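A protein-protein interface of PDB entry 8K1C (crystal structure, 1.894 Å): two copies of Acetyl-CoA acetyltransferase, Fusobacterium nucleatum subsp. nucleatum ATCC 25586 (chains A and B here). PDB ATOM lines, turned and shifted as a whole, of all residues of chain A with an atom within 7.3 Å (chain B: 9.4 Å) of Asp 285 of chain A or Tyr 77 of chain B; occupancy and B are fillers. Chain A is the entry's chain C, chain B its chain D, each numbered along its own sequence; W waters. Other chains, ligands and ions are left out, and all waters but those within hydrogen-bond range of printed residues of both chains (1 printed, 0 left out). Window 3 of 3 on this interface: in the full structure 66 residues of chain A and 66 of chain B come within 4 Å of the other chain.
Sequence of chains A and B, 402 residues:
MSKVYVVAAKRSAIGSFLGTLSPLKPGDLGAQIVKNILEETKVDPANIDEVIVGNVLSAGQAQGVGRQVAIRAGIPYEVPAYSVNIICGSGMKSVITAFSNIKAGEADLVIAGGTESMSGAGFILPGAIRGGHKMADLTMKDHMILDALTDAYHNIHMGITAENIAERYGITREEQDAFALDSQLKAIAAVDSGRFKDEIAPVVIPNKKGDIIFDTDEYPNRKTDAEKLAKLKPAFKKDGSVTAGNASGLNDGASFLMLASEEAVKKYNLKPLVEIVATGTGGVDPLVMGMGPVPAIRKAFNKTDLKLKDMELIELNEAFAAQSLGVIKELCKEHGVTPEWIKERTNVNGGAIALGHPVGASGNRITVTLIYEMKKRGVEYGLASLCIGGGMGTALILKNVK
OH of Tyr 153 of chain A lies close to O of Arg 67 of chain B (3.2 Å).
The backbone NH (N) of Gln 68 of chain B lies within hydrogen-bond range of the side-chain hydroxyl (OH) of Tyr 153 of chain A (3.0 Å).
The guanidinium group (NH2) of Arg 67 of chain B lies within hydrogen-bond range of the backbone carbonyl oxygen (O) of Val 284 of chain A.
O of Gly 390 of chain A sits at hydrogen-bond distance from NE of Arg 67 of chain B, at 3.1 Å.
NH2 of Arg 67 of chain B is in hydrogen-bond range of O of Gly 391 of chain A (3.0 Å).
SD of Met 392 of chain A is in hydrogen-bond range of N of Ala 81 of chain B (3.4 Å).
The side-chain carboxylate of Asp 151 of chain A is in hydrogen-bond range of the backbone NH of Tyr 153 of chain A (3.0 Å).
N of Val 284 of chain A lies within hydrogen-bond range of O of Gly 391 of chain A, at 2.8 Å.
N of Leu 287 of chain A lies within hydrogen-bond range of OD1 of Asp 285 of chain A (2.9 Å).
NH2 of Arg 67 of chain B sits at hydrogen-bond distance from O of Tyr 77 of chain B (2.9 Å).
NH1 of Arg 67 of chain B sits at hydrogen-bond distance from O of Val 79 of chain B, 2.7 Å away.
The guanidinium group of Arg 72 of chain B sits at hydrogen-bond distance from the side-chain amide oxygen of Gln 68 of chain B, 3.0 Å away.
Among the printed residues, pairs that only touch across the chains: Gly 283 of chain A with Tyr 77 of chain B (3.3 Å), Val 284 of chain A with Tyr 77 of chain B (3.3 Å), Asp 285 of chain A with Tyr 77 of chain B (3.6 Å), Pro 286 of chain A with Tyr 77 of chain B (3.6 Å), Tyr 153 of chain A with Ile 71 of chain B (3.6 Å), Gly 283 of chain A with Glu 78 of chain B (3.7 Å), Met 392 of chain A with Pro 80 of chain B (3.8 Å), Tyr 153 of chain A with Arg 72 of chain B (3.9 Å) and Met 392 of chain A with Arg 67 of chain B (3.9 Å).
His 154 of chain A touches none of the printed residues of chain B.
Of chain B, only Tyr 77 (3.3 Å) and Glu 78 (3.7 Å) come within 4 Å of Gly 283 of chain A.
Of chain B, only Tyr 77 comes within 4 Å of Asp 285 of chain A.
Of chain B, only Tyr 77 comes within 4 Å of Pro 286 of chain A.
Val 288 of chain A touches none of the printed residues of chain B.
Of the printed residues of chain A, Arg 72 of chain B touches Tyr 153 (3.9 Å).
Of the printed residues of chain A, Pro 80 of chain B touches Met 392 (3.8 Å).
Of the printed residues of chain A, Ala 81 of chain B touches Met 392.
The nearest residue of chain B that does not touch Asp 285 of chain A is Arg 67 of chain B (5.5 Å).
The nearest residue of chain A that does not touch Tyr 77 of chain B is Gly 391 of chain A (4.04 Å).
Printed residues of chain A that touch a printed residue of chain B: Tyr 153, Gly 283, Val 284, Asp 285, Pro 286, Gly 390, Gly 391 and Met 392.
No position is printed for both chains.
Of the 15 pairs that touch across the chains among the printed residues, none has its exchanged pair printed and touching as well.
Water W1 bridges O of Glu 78 of chain B (2.6 Å) and N of Gly 283 of chain A (2.9 Å).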
ATOM      1  N   ASP A 151      22.150 -11.664  -9.349  1.00  0.00           N
ATOM      2  CA  ASP A 151      22.179 -10.295  -8.855  1.00  0.00           C
ATOM      3  C   ASP A 151      20.886  -9.574  -9.210  1.00  0.00           C
ATOM      4  O   ASP A 151      20.364  -9.712 -10.320  1.00  0.00           O
ATOM      5  CB  ASP A 151      23.370  -9.535  -9.441  1.00  0.00           C
ATOM      6  CG  ASP A 151      23.416  -8.109  -8.962  1.00  0.00           C
ATOM      7  OD1 ASP A 151      23.712  -7.903  -7.759  1.00  0.00           O
ATOM      8  OD2 ASP A 151      23.100  -7.206  -9.773  1.00  0.00           O
ATOM      9  N   TYR A 153      20.261  -6.373  -9.533  1.00  0.00           N
ATOM     10  CA  TYR A 153      20.467  -5.086 -10.190  1.00  0.00           C
ATOM     11  C   TYR A 153      20.999  -5.209 -11.603  1.00  0.00           C
ATOM     12  O   TYR A 153      20.633  -4.404 -12.457  1.00  0.00           O
ATOM     13  CB  TYR A 153      21.422  -4.225  -9.346  1.00  0.00           C
ATOM     14  CG  TYR A 153      21.055  -4.428  -7.910  1.00  0.00           C
ATOM     15  CD1 TYR A 153      19.848  -3.926  -7.421  1.00  0.00           C
ATOM     16  CD2 TYR A 153      21.843  -5.198  -7.068  1.00  0.00           C
ATOM     17  CE1 TYR A 153      19.456  -4.154  -6.131  1.00  0.00           C
ATOM     18  CE2 TYR A 153      21.452  -5.436  -5.771  1.00  0.00           C
ATOM     19  CZ  TYR A 153      20.254  -4.911  -5.309  1.00  0.00           C
ATOM     20  OH  TYR A 153      19.843  -5.135  -4.023  1.00  0.00           O
ATOM     21  N   HIS A 154      21.816  -6.218 -11.887  1.00  0.00           N
ATOM     22  CA  HIS A 154      22.309  -6.421 -13.234  1.00  0.00           C
ATOM     23  C   HIS A 154      21.854  -7.733 -13.842  1.00  0.00           C
ATOM     24  O   HIS A 154      22.241  -8.031 -14.980  1.00  0.00           O
ATOM     25  CB  HIS A 154      23.834  -6.350 -13.250  1.00  0.00           C
ATOM     26  CG  HIS A 154      24.374  -5.087 -12.678  1.00  0.00           C
ATOM     27  ND1 HIS A 154      24.454  -3.921 -13.404  1.00  0.00           N
ATOM     28  CD2 HIS A 154      24.855  -4.802 -11.446  1.00  0.00           C
ATOM     29  CE1 HIS A 154      24.970  -2.970 -12.644  1.00  0.00           C
ATOM     30  NE2 HIS A 154      25.226  -3.481 -11.454  1.00  0.00           N
ATOM     31  N   THR A 161      30.169 -11.951 -11.812  1.00  0.00           N
ATOM     32  CA  THR A 161      30.881 -11.027 -10.884  1.00  0.00           C
ATOM     33  C   THR A 161      32.299 -11.564 -10.652  1.00  0.00           C
ATOM     34  O   THR A 161      33.160 -10.797 -10.431  1.00  0.00           O
ATOM     35  CB  THR A 161      30.122 -10.757  -9.579  1.00  0.00           C
ATOM     36  OG1 THR A 161      30.252 -11.860  -8.702  1.00  0.00           O
ATOM     37  CG2 THR A 161      28.680 -10.365  -9.795  1.00  0.00           C
ATOM     38  N   ARG A 168      39.305  -7.076 -13.685  1.00  0.00           N
ATOM     39  CA  ARG A 168      39.777  -5.826 -13.091  1.00  0.00           C
ATOM     40  C   ARG A 168      41.107  -5.990 -12.361  1.00  0.00           C
ATOM     41  O   ARG A 168      41.936  -5.078 -12.381  1.00  0.00           O
ATOM     42  CB  ARG A 168      38.717  -5.267 -12.139  1.00  0.00           C
ATOM     43  CG  ARG A 168      37.425  -4.840 -12.843  1.00  0.00           C
ATOM     44  CD  ARG A 168      36.578  -3.986 -11.931  1.00  0.00           C
ATOM     45  NE  ARG A 168      35.217  -3.794 -12.412  1.00  0.00           N
ATOM     46  CZ  ARG A 168      34.382  -2.921 -11.861  1.00  0.00           C
ATOM     47  NH1 ARG A 168      34.798  -2.184 -10.839  1.00  0.00           N
ATOM     48  NH2 ARG A 168      33.146  -2.778 -12.325  1.00  0.00           N
ATOM     49  N   GLY A 282      30.403  -5.259   5.643  1.00  0.00           N
ATOM     50  CA  GLY A 282      30.833  -4.269   4.684  1.00  0.00           C
ATOM     51  C   GLY A 282      30.032  -4.360   3.395  1.00  0.00           C
ATOM     52  O   GLY A 282      29.306  -5.333   3.151  1.00  0.00           O
ATOM     53  N   GLY A 283      30.193  -3.335   2.563  1.00  0.00           N
ATOM     54  CA  GLY A 283      29.517  -3.285   1.277  1.00  0.00           C
ATOM     55  C   GLY A 283      30.461  -2.828   0.182  1.00  0.00           C
ATOM     56  O   GLY A 283      31.387  -2.049   0.417  1.00  0.00           O
ATOM     57  N   VAL A 284      30.228  -3.354  -1.030  1.00  0.00           N
ATOM     58  CA  VAL A 284      30.991  -3.029  -2.236  1.00  0.00           C
ATOM     59  C   VAL A 284      30.016  -2.996  -3.410  1.00  0.00           C
ATOM     60  O   VAL A 284      28.812  -3.213  -3.252  1.00  0.00           O
ATOM     61  CB  VAL A 284      32.125  -4.043  -2.512  1.00  0.00           C
ATOM     62  CG1 VAL A 284      33.055  -4.147  -1.348  1.00  0.00           C
ATOM     63  CG2 VAL A 284      31.543  -5.401  -2.844  1.00  0.00           C
ATOM     64  N   ASP A 285      30.543  -2.755  -4.600  1.00  0.00           N
ATOM     65  CA  ASP A 285      29.714  -2.755  -5.800  1.00  0.00           C
ATOM     66  C   ASP A 285      29.187  -4.162  -6.074  1.00  0.00           C
ATOM     67  O   ASP A 285      29.964  -5.124  -6.047  1.00  0.00           O
ATOM     68  CB  ASP A 285      30.524  -2.238  -6.991  1.00  0.00           C
ATOM     69  CG  ASP A 285      29.655  -1.867  -8.181  1.00  0.00           C
ATOM     70  OD1 ASP A 285      28.774  -2.673  -8.565  1.00  0.00           O
ATOM     71  OD2 ASP A 285      29.851  -0.757  -8.729  1.00  0.00           O
ATOM     72  N   PRO A 286      27.881  -4.328  -6.314  1.00  0.00           N
ATOM     73  CA  PRO A 286      27.365  -5.660  -6.688  1.00  0.00           C
ATOM     74  C   PRO A 286      28.126  -6.314  -7.832  1.00  0.00           C
ATOM     75  O   PRO A 286      28.319  -7.536  -7.822  1.00  0.00           O
ATOM     76  CB  PRO A 286      25.910  -5.372  -7.078  1.00  0.00           C
ATOM     77  CG  PRO A 286      25.545  -4.141  -6.304  1.00  0.00           C
ATOM     78  CD  PRO A 286      26.809  -3.333  -6.139  1.00  0.00           C
ATOM     79  N   LEU A 287      28.582  -5.543  -8.810  1.00  0.00           N
ATOM     80  CA  LEU A 287      29.346  -6.045  -9.980  1.00  0.00           C
ATOM     81  C   LEU A 287      30.629  -6.766  -9.557  1.00  0.00           C
ATOM     82  O   LEU A 287      31.132  -7.564 -10.310  1.00  0.00           O
ATOM     83  CB  LEU A 287      29.702  -4.856 -10.868  1.00  0.00           C
ATOM     84  CG  LEU A 287      28.531  -4.274 -11.641  1.00  0.00           C
ATOM     85  CD1 LEU A 287      28.921  -2.969 -12.298  1.00  0.00           C
ATOM     86  CD2 LEU A 287      28.031  -5.262 -12.686  1.00  0.00           C
ATOM     87  N   VAL A 288      31.123  -6.449  -8.358  1.00  0.00           N
ATOM     88  CA  VAL A 288      32.349  -7.117  -7.828  1.00  0.00           C
ATOM     89  C   VAL A 288      32.033  -7.626  -6.420  1.00  0.00           C
ATOM     90  O   VAL A 288      32.890  -7.466  -5.528  1.00  0.00           O
ATOM     91  CB  VAL A 288      33.560  -6.164  -7.838  1.00  0.00           C
ATOM     92  CG1 VAL A 288      34.238  -6.128  -9.200  1.00  0.00           C
ATOM     93  CG2 VAL A 288      33.176  -4.761  -7.397  1.00  0.00           C
ATOM     94  N   MET A 289      30.849  -8.221  -6.232  1.00  0.00           N
ATOM     95  CA  MET A 289      30.436  -8.758  -4.906  1.00  0.00           C
ATOM     96  C   MET A 289      31.647  -9.354  -4.183  1.00  0.00           C
ATOM     97  O   MET A 289      31.827  -9.043  -2.987  1.00  0.00           O
ATOM     98  CB  MET A 289      29.387  -9.862  -5.072  1.00  0.00           C
ATOM     99  CG  MET A 289      29.555 -10.998  -4.076  1.00  0.00           C
ATOM    100  SD  MET A 289      29.155 -12.652  -4.690  1.00  0.00           S
ATOM    101  CE  MET A 289      30.727 -13.155  -5.386  1.00  0.00           C
ATOM    102  N   GLY A 290      32.456 -10.154  -4.884  1.00  0.00           N
ATOM    103  CA  GLY A 290      33.592 -10.851  -4.250  1.00  0.00           C
ATOM    104  C   GLY A 290      34.466  -9.972  -3.375  1.00  0.00           C
ATOM    105  O   GLY A 290      35.115 -10.527  -2.477  1.00  0.00           O
ATOM    106  N   MET A 291      34.513  -8.664  -3.634  1.00  0.00           N
ATOM    107  CA  MET A 291      35.423  -7.774  -2.867  1.00  0.00           C
ATOM    108  C   MET A 291      34.810  -7.445  -1.502  1.00  0.00           C
ATOM    109  O   MET A 291      35.400  -6.614  -0.786  1.00  0.00           O
ATOM    110  CB  MET A 291      35.683  -6.476  -3.637  1.00  0.00           C
ATOM    111  CG  MET A 291      36.413  -6.699  -4.946  1.00  0.00           C
ATOM    112  SD  MET A 291      37.611  -8.054  -4.842  1.00  0.00           S
ATOM    113  CE  MET A 291      38.889  -7.287  -3.849  1.00  0.00           C
ATOM    114  N   GLY A 292      33.691  -8.082  -1.142  1.00  0.00           N
ATOM    115  CA  GLY A 292      33.037  -7.746   0.105  1.00  0.00           C
ATOM    116  C   GLY A 292      33.815  -8.009   1.387  1.00  0.00           C
ATOM    117  O   GLY A 292      33.657  -7.272   2.365  1.00  0.00           O
ATOM    118  N   ILE A 388      29.424 -11.795  -0.337  1.00  0.00           N
ATOM    119  CA  ILE A 388      27.963 -11.880  -0.232  1.00  0.00           C
ATOM    120  C   ILE A 388      27.312 -11.342  -1.501  1.00  0.00           C
ATOM    121  O   ILE A 388      27.549 -10.187  -1.884  1.00  0.00           O
ATOM    122  CB  ILE A 388      27.470 -11.085   0.992  1.00  0.00           C
ATOM    123  CG1 ILE A 388      28.016 -11.673   2.297  1.00  0.00           C
ATOM    124  CG2 ILE A 388      25.938 -10.998   1.017  1.00  0.00           C
ATOM    125  CD1 ILE A 388      27.555 -10.914   3.544  1.00  0.00           C
ATOM    126  N   GLY A 390      25.155  -9.445  -4.059  1.00  0.00           N
ATOM    127  CA  GLY A 390      24.669  -8.092  -3.886  1.00  0.00           C
ATOM    128  C   GLY A 390      25.714  -7.097  -3.418  1.00  0.00           C
ATOM    129  O   GLY A 390      25.395  -5.905  -3.285  1.00  0.00           O
ATOM    130  N   GLY A 391      26.939  -7.545  -3.146  1.00  0.00           N
ATOM    131  CA  GLY A 391      28.037  -6.658  -2.834  1.00  0.00           C
ATOM    132  C   GLY A 391      28.216  -6.353  -1.361  1.00  0.00           C
ATOM    133  O   GLY A 391      28.168  -5.184  -0.954  1.00  0.00           O
ATOM    134  N   MET A 392      28.430  -7.394  -0.554  1.00  0.00           N
ATOM    135  CA  MET A 392      28.574  -7.245   0.883  1.00  0.00           C
ATOM    136  C   MET A 392      29.580  -8.282   1.362  1.00  0.00           C
ATOM    137  O   MET A 392      30.000  -9.167   0.619  1.00  0.00           O
ATOM    138  CB  MET A 392      27.211  -7.414   1.602  1.00  0.00           C
ATOM    139  CG  MET A 392      26.184  -6.290   1.343  1.00  0.00           C
ATOM    140  SD  MET A 392      24.593  -6.482   2.197  1.00  0.00           S
ATOM    141  CE  MET A 392      23.842  -7.450   0.867  1.00  0.00           C
ATOM    142  N   PRO B  45      22.739   9.583   2.971  1.00  0.00           N
ATOM    143  CA  PRO B  45      22.579   8.121   3.114  1.00  0.00           C
ATOM    144  C   PRO B  45      23.869   7.382   3.460  1.00  0.00           C
ATOM    145  O   PRO B  45      23.797   6.269   4.001  1.00  0.00           O
ATOM    146  CB  PRO B  45      22.041   7.681   1.745  1.00  0.00           C
ATOM    147  CG  PRO B  45      21.559   8.917   1.081  1.00  0.00           C
ATOM    148  CD  PRO B  45      22.297  10.083   1.660  1.00  0.00           C
ATOM    149  N   ALA B  46      25.043   7.963   3.168  1.00  0.00           N
ATOM    150  CA  ALA B  46      26.320   7.334   3.492  1.00  0.00           C
ATOM    151  C   ALA B  46      26.563   7.229   4.990  1.00  0.00           C
ATOM    152  O   ALA B  46      27.461   6.481   5.407  1.00  0.00           O
ATOM    153  CB  ALA B  46      27.471   8.116   2.854  1.00  0.00           C
ATOM    154  N   ILE B  48      24.245   6.121   7.099  1.00  0.00           N
ATOM    155  CA  ILE B  48      23.466   5.016   7.648  1.00  0.00           C
ATOM    156  C   ILE B  48      24.388   3.822   7.847  1.00  0.00           C
ATOM    157  O   ILE B  48      25.197   3.498   6.970  1.00  0.00           O
ATOM    158  CB  ILE B  48      22.284   4.665   6.727  1.00  0.00           C
ATOM    159  CG1 ILE B  48      21.341   5.854   6.584  1.00  0.00           C
ATOM    160  CG2 ILE B  48      21.508   3.472   7.271  1.00  0.00           C
ATOM    161  CD1 ILE B  48      20.340   5.647   5.488  1.00  0.00           C
ATOM    162  N   ASP B  49      24.267   3.162   9.007  1.00  0.00           N
ATOM    163  CA  ASP B  49      25.085   1.985   9.283  1.00  0.00           C
ATOM    164  C   ASP B  49      24.546   0.735   8.596  1.00  0.00           C
ATOM    165  O   ASP B  49      25.325  -0.093   8.116  1.00  0.00           O
ATOM    166  CB  ASP B  49      25.191   1.762  10.789  1.00  0.00           C
ATOM    167  CG  ASP B  49      26.047   2.819  11.464  1.00  0.00           C
ATOM    168  OD1 ASP B  49      27.261   2.903  11.162  1.00  0.00           O
ATOM    169  OD2 ASP B  49      25.497   3.595  12.268  1.00  0.00           O
ATOM    170  N   ARG B  67      18.334  -5.741   0.571  1.00  0.00           N
ATOM    171  CA  ARG B  67      19.324  -4.929  -0.127  1.00  0.00           C
ATOM    172  C   ARG B  67      18.712  -4.192  -1.317  1.00  0.00           C
ATOM    173  O   ARG B  67      19.135  -3.073  -1.633  1.00  0.00           O
ATOM    174  CB  ARG B  67      20.499  -5.812  -0.556  1.00  0.00           C
ATOM    175  CG  ARG B  67      21.557  -5.158  -1.456  1.00  0.00           C
ATOM    176  CD  ARG B  67      22.467  -4.148  -0.733  1.00  0.00           C
ATOM    177  NE  ARG B  67      23.787  -4.093  -1.368  1.00  0.00           N
ATOM    178  CZ  ARG B  67      24.782  -3.304  -0.967  1.00  0.00           C
ATOM    179  NH1 ARG B  67      24.602  -2.489   0.069  1.00  0.00           N
ATOM    180  NH2 ARG B  67      25.959  -3.335  -1.595  1.00  0.00           N
ATOM    181  N   GLN B  68      17.703  -4.773  -1.975  1.00  0.00           N
ATOM    182  CA  GLN B  68      17.038  -4.043  -3.047  1.00  0.00           C
ATOM    183  C   GLN B  68      16.367  -2.787  -2.514  1.00  0.00           C
ATOM    184  O   GLN B  68      16.353  -1.749  -3.187  1.00  0.00           O
ATOM    185  CB  GLN B  68      16.006  -4.922  -3.741  1.00  0.00           C
ATOM    186  CG  GLN B  68      16.581  -6.131  -4.446  1.00  0.00           C
ATOM    187  CD  GLN B  68      15.483  -7.095  -4.836  1.00  0.00           C
ATOM    188  OE1 GLN B  68      14.382  -6.680  -5.197  1.00  0.00           O
ATOM    189  NE2 GLN B  68      15.759  -8.391  -4.726  1.00  0.00           N
ATOM    190  N   ALA B  70      17.340  -0.895  -0.077  1.00  0.00           N
ATOM    191  CA  ALA B  70      18.341   0.128   0.188  1.00  0.00           C
ATOM    192  C   ALA B  70      18.875   0.723  -1.105  1.00  0.00           C
ATOM    193  O   ALA B  70      18.946   1.947  -1.251  1.00  0.00           O
ATOM    194  CB  ALA B  70      19.478  -0.456   1.027  1.00  0.00           C
ATOM    195  N   ILE B  71      19.246  -0.125  -2.069  1.00  0.00           N
ATOM    196  CA  ILE B  71      19.912   0.391  -3.263  1.00  0.00           C
ATOM    197  C   ILE B  71      18.940   1.191  -4.125  1.00  0.00           C
ATOM    198  O   ILE B  71      19.285   2.256  -4.651  1.00  0.00           O
ATOM    199  CB  ILE B  71      20.561  -0.760  -4.051  1.00  0.00           C
ATOM    200  CG1 ILE B  71      21.749  -1.310  -3.271  1.00  0.00           C
ATOM    201  CG2 ILE B  71      21.001  -0.277  -5.425  1.00  0.00           C
ATOM    202  CD1 ILE B  71      22.498  -2.335  -4.036  1.00  0.00           C
ATOM    203  N   ARG B  72      17.702   0.720  -4.255  1.00  0.00           N
ATOM    204  CA  ARG B  72      16.758   1.455  -5.087  1.00  0.00           C
ATOM    205  C   ARG B  72      16.260   2.730  -4.420  1.00  0.00           C
ATOM    206  O   ARG B  72      15.698   3.591  -5.108  1.00  0.00           O
ATOM    207  CB  ARG B  72      15.604   0.538  -5.478  1.00  0.00           C
ATOM    208  CG  ARG B  72      16.114  -0.790  -6.048  1.00  0.00           C
ATOM    209  CD  ARG B  72      15.190  -1.474  -7.034  1.00  0.00           C
ATOM    210  NE  ARG B  72      15.843  -2.681  -7.543  1.00  0.00           N
ATOM    211  CZ  ARG B  72      15.368  -3.921  -7.415  1.00  0.00           C
ATOM    212  NH1 ARG B  72      14.199  -4.149  -6.816  1.00  0.00           N
ATOM    213  NH2 ARG B  72      16.067  -4.942  -7.902  1.00  0.00           N
ATOM    214  N   GLY B  74      18.449   4.780  -3.097  1.00  0.00           N
ATOM    215  CA  GLY B  74      19.591   5.661  -3.176  1.00  0.00           C
ATOM    216  C   GLY B  74      20.594   5.514  -2.055  1.00  0.00           C
ATOM    217  O   GLY B  74      21.459   6.380  -1.908  1.00  0.00           O
ATOM    218  N   ILE B  75      20.511   4.461  -1.259  1.00  0.00           N
ATOM    219  CA  ILE B  75      21.519   4.238  -0.223  1.00  0.00           C
ATOM    220  C   ILE B  75      22.750   3.605  -0.869  1.00  0.00           C
ATOM    221  O   ILE B  75      22.605   2.638  -1.637  1.00  0.00           O
ATOM    222  CB  ILE B  75      20.949   3.362   0.884  1.00  0.00           C
ATOM    223  CG1 ILE B  75      19.687   4.043   1.445  1.00  0.00           C
ATOM    224  CG2 ILE B  75      21.994   3.073   1.965  1.00  0.00           C
ATOM    225  CD1 ILE B  75      19.146   3.408   2.690  1.00  0.00           C
ATOM    226  N   PRO B  76      23.954   4.131  -0.614  1.00  0.00           N
ATOM    227  CA  PRO B  76      25.142   3.685  -1.366  1.00  0.00           C
ATOM    228  C   PRO B  76      25.554   2.257  -1.029  1.00  0.00           C
ATOM    229  O   PRO B  76      25.205   1.711   0.021  1.00  0.00           O
ATOM    230  CB  PRO B  76      26.235   4.687  -0.964  1.00  0.00           C
ATOM    231  CG  PRO B  76      25.708   5.457   0.212  1.00  0.00           C
ATOM    232  CD  PRO B  76      24.211   5.333   0.207  1.00  0.00           C
ATOM    233  N   TYR B  77      26.324   1.664  -1.960  1.00  0.00           N
ATOM    234  CA  TYR B  77      26.685   0.242  -1.903  1.00  0.00           C
ATOM    235  C   TYR B  77      27.412  -0.125  -0.625  1.00  0.00           C
ATOM    236  O   TYR B  77      27.383  -1.292  -0.208  1.00  0.00           O
ATOM    237  CB  TYR B  77      27.593  -0.134  -3.072  1.00  0.00           C
ATOM    238  CG  TYR B  77      26.991   0.052  -4.427  1.00  0.00           C
ATOM    239  CD1 TYR B  77      25.649  -0.224  -4.658  1.00  0.00           C
ATOM    240  CD2 TYR B  77      27.767   0.504  -5.491  1.00  0.00           C
ATOM    241  CE1 TYR B  77      25.094  -0.052  -5.922  1.00  0.00           C
ATOM    242  CE2 TYR B  77      27.221   0.673  -6.752  1.00  0.00           C
ATOM    243  CZ  TYR B  77      25.890   0.396  -6.959  1.00  0.00           C
ATOM    244  OH  TYR B  77      25.351   0.567  -8.205  1.00  0.00           O
ATOM    245  N   GLU B  78      28.114   0.836  -0.023  1.00  0.00           N
ATOM    246  CA  GLU B  78      28.921   0.595   1.159  1.00  0.00           C
ATOM    247  C   GLU B  78      28.080   0.351   2.398  1.00  0.00           C
ATOM    248  O   GLU B  78      28.618  -0.142   3.392  1.00  0.00           O
ATOM    249  CB  GLU B  78      29.864   1.783   1.395  1.00  0.00           C
ATOM    250  CG  GLU B  78      30.953   1.951   0.318  1.00  0.00           C
ATOM    251  CD  GLU B  78      30.437   2.626  -0.951  1.00  0.00           C
ATOM    252  OE1 GLU B  78      29.515   3.453  -0.844  1.00  0.00           O
ATOM    253  OE2 GLU B  78      30.935   2.317  -2.053  1.00  0.00           O
ATOM    254  N   VAL B  79      26.787   0.669   2.362  1.00  0.00           N
ATOM    255  CA  VAL B  79      25.889   0.445   3.493  1.00  0.00           C
ATOM    256  C   VAL B  79      25.247  -0.929   3.312  1.00  0.00           C
ATOM    257  O   VAL B  79      24.495  -1.124   2.339  1.00  0.00           O
ATOM    258  CB  VAL B  79      24.826   1.543   3.603  1.00  0.00           C
ATOM    259  CG1 VAL B  79      23.946   1.314   4.830  1.00  0.00           C
ATOM    260  CG2 VAL B  79      25.492   2.899   3.679  1.00  0.00           C
ATOM    261  N   PRO B  80      25.527  -1.891   4.181  1.00  0.00           N
ATOM    262  CA  PRO B  80      24.906  -3.208   4.032  1.00  0.00           C
ATOM    263  C   PRO B  80      23.415  -3.148   4.339  1.00  0.00           C
ATOM    264  O   PRO B  80      22.927  -2.283   5.083  1.00  0.00           O
ATOM    265  CB  PRO B  80      25.656  -4.076   5.043  1.00  0.00           C
ATOM    266  CG  PRO B  80      26.310  -3.129   5.991  1.00  0.00           C
ATOM    267  CD  PRO B  80      26.556  -1.861   5.239  1.00  0.00           C
ATOM    268  N   ALA B  81      22.683  -4.071   3.712  1.00  0.00           N
ATOM    269  CA  ALA B  81      21.239  -4.157   3.843  1.00  0.00           C
ATOM    270  C   ALA B  81      20.835  -5.608   3.635  1.00  0.00           C
ATOM    271  O   ALA B  81      21.375  -6.284   2.757  1.00  0.00           O
ATOM    272  CB  ALA B  81      20.525  -3.246   2.837  1.00  0.00           C
HETATM  273  O   HOH W   1      30.907  -0.963   4.161  1.00  0.00           O
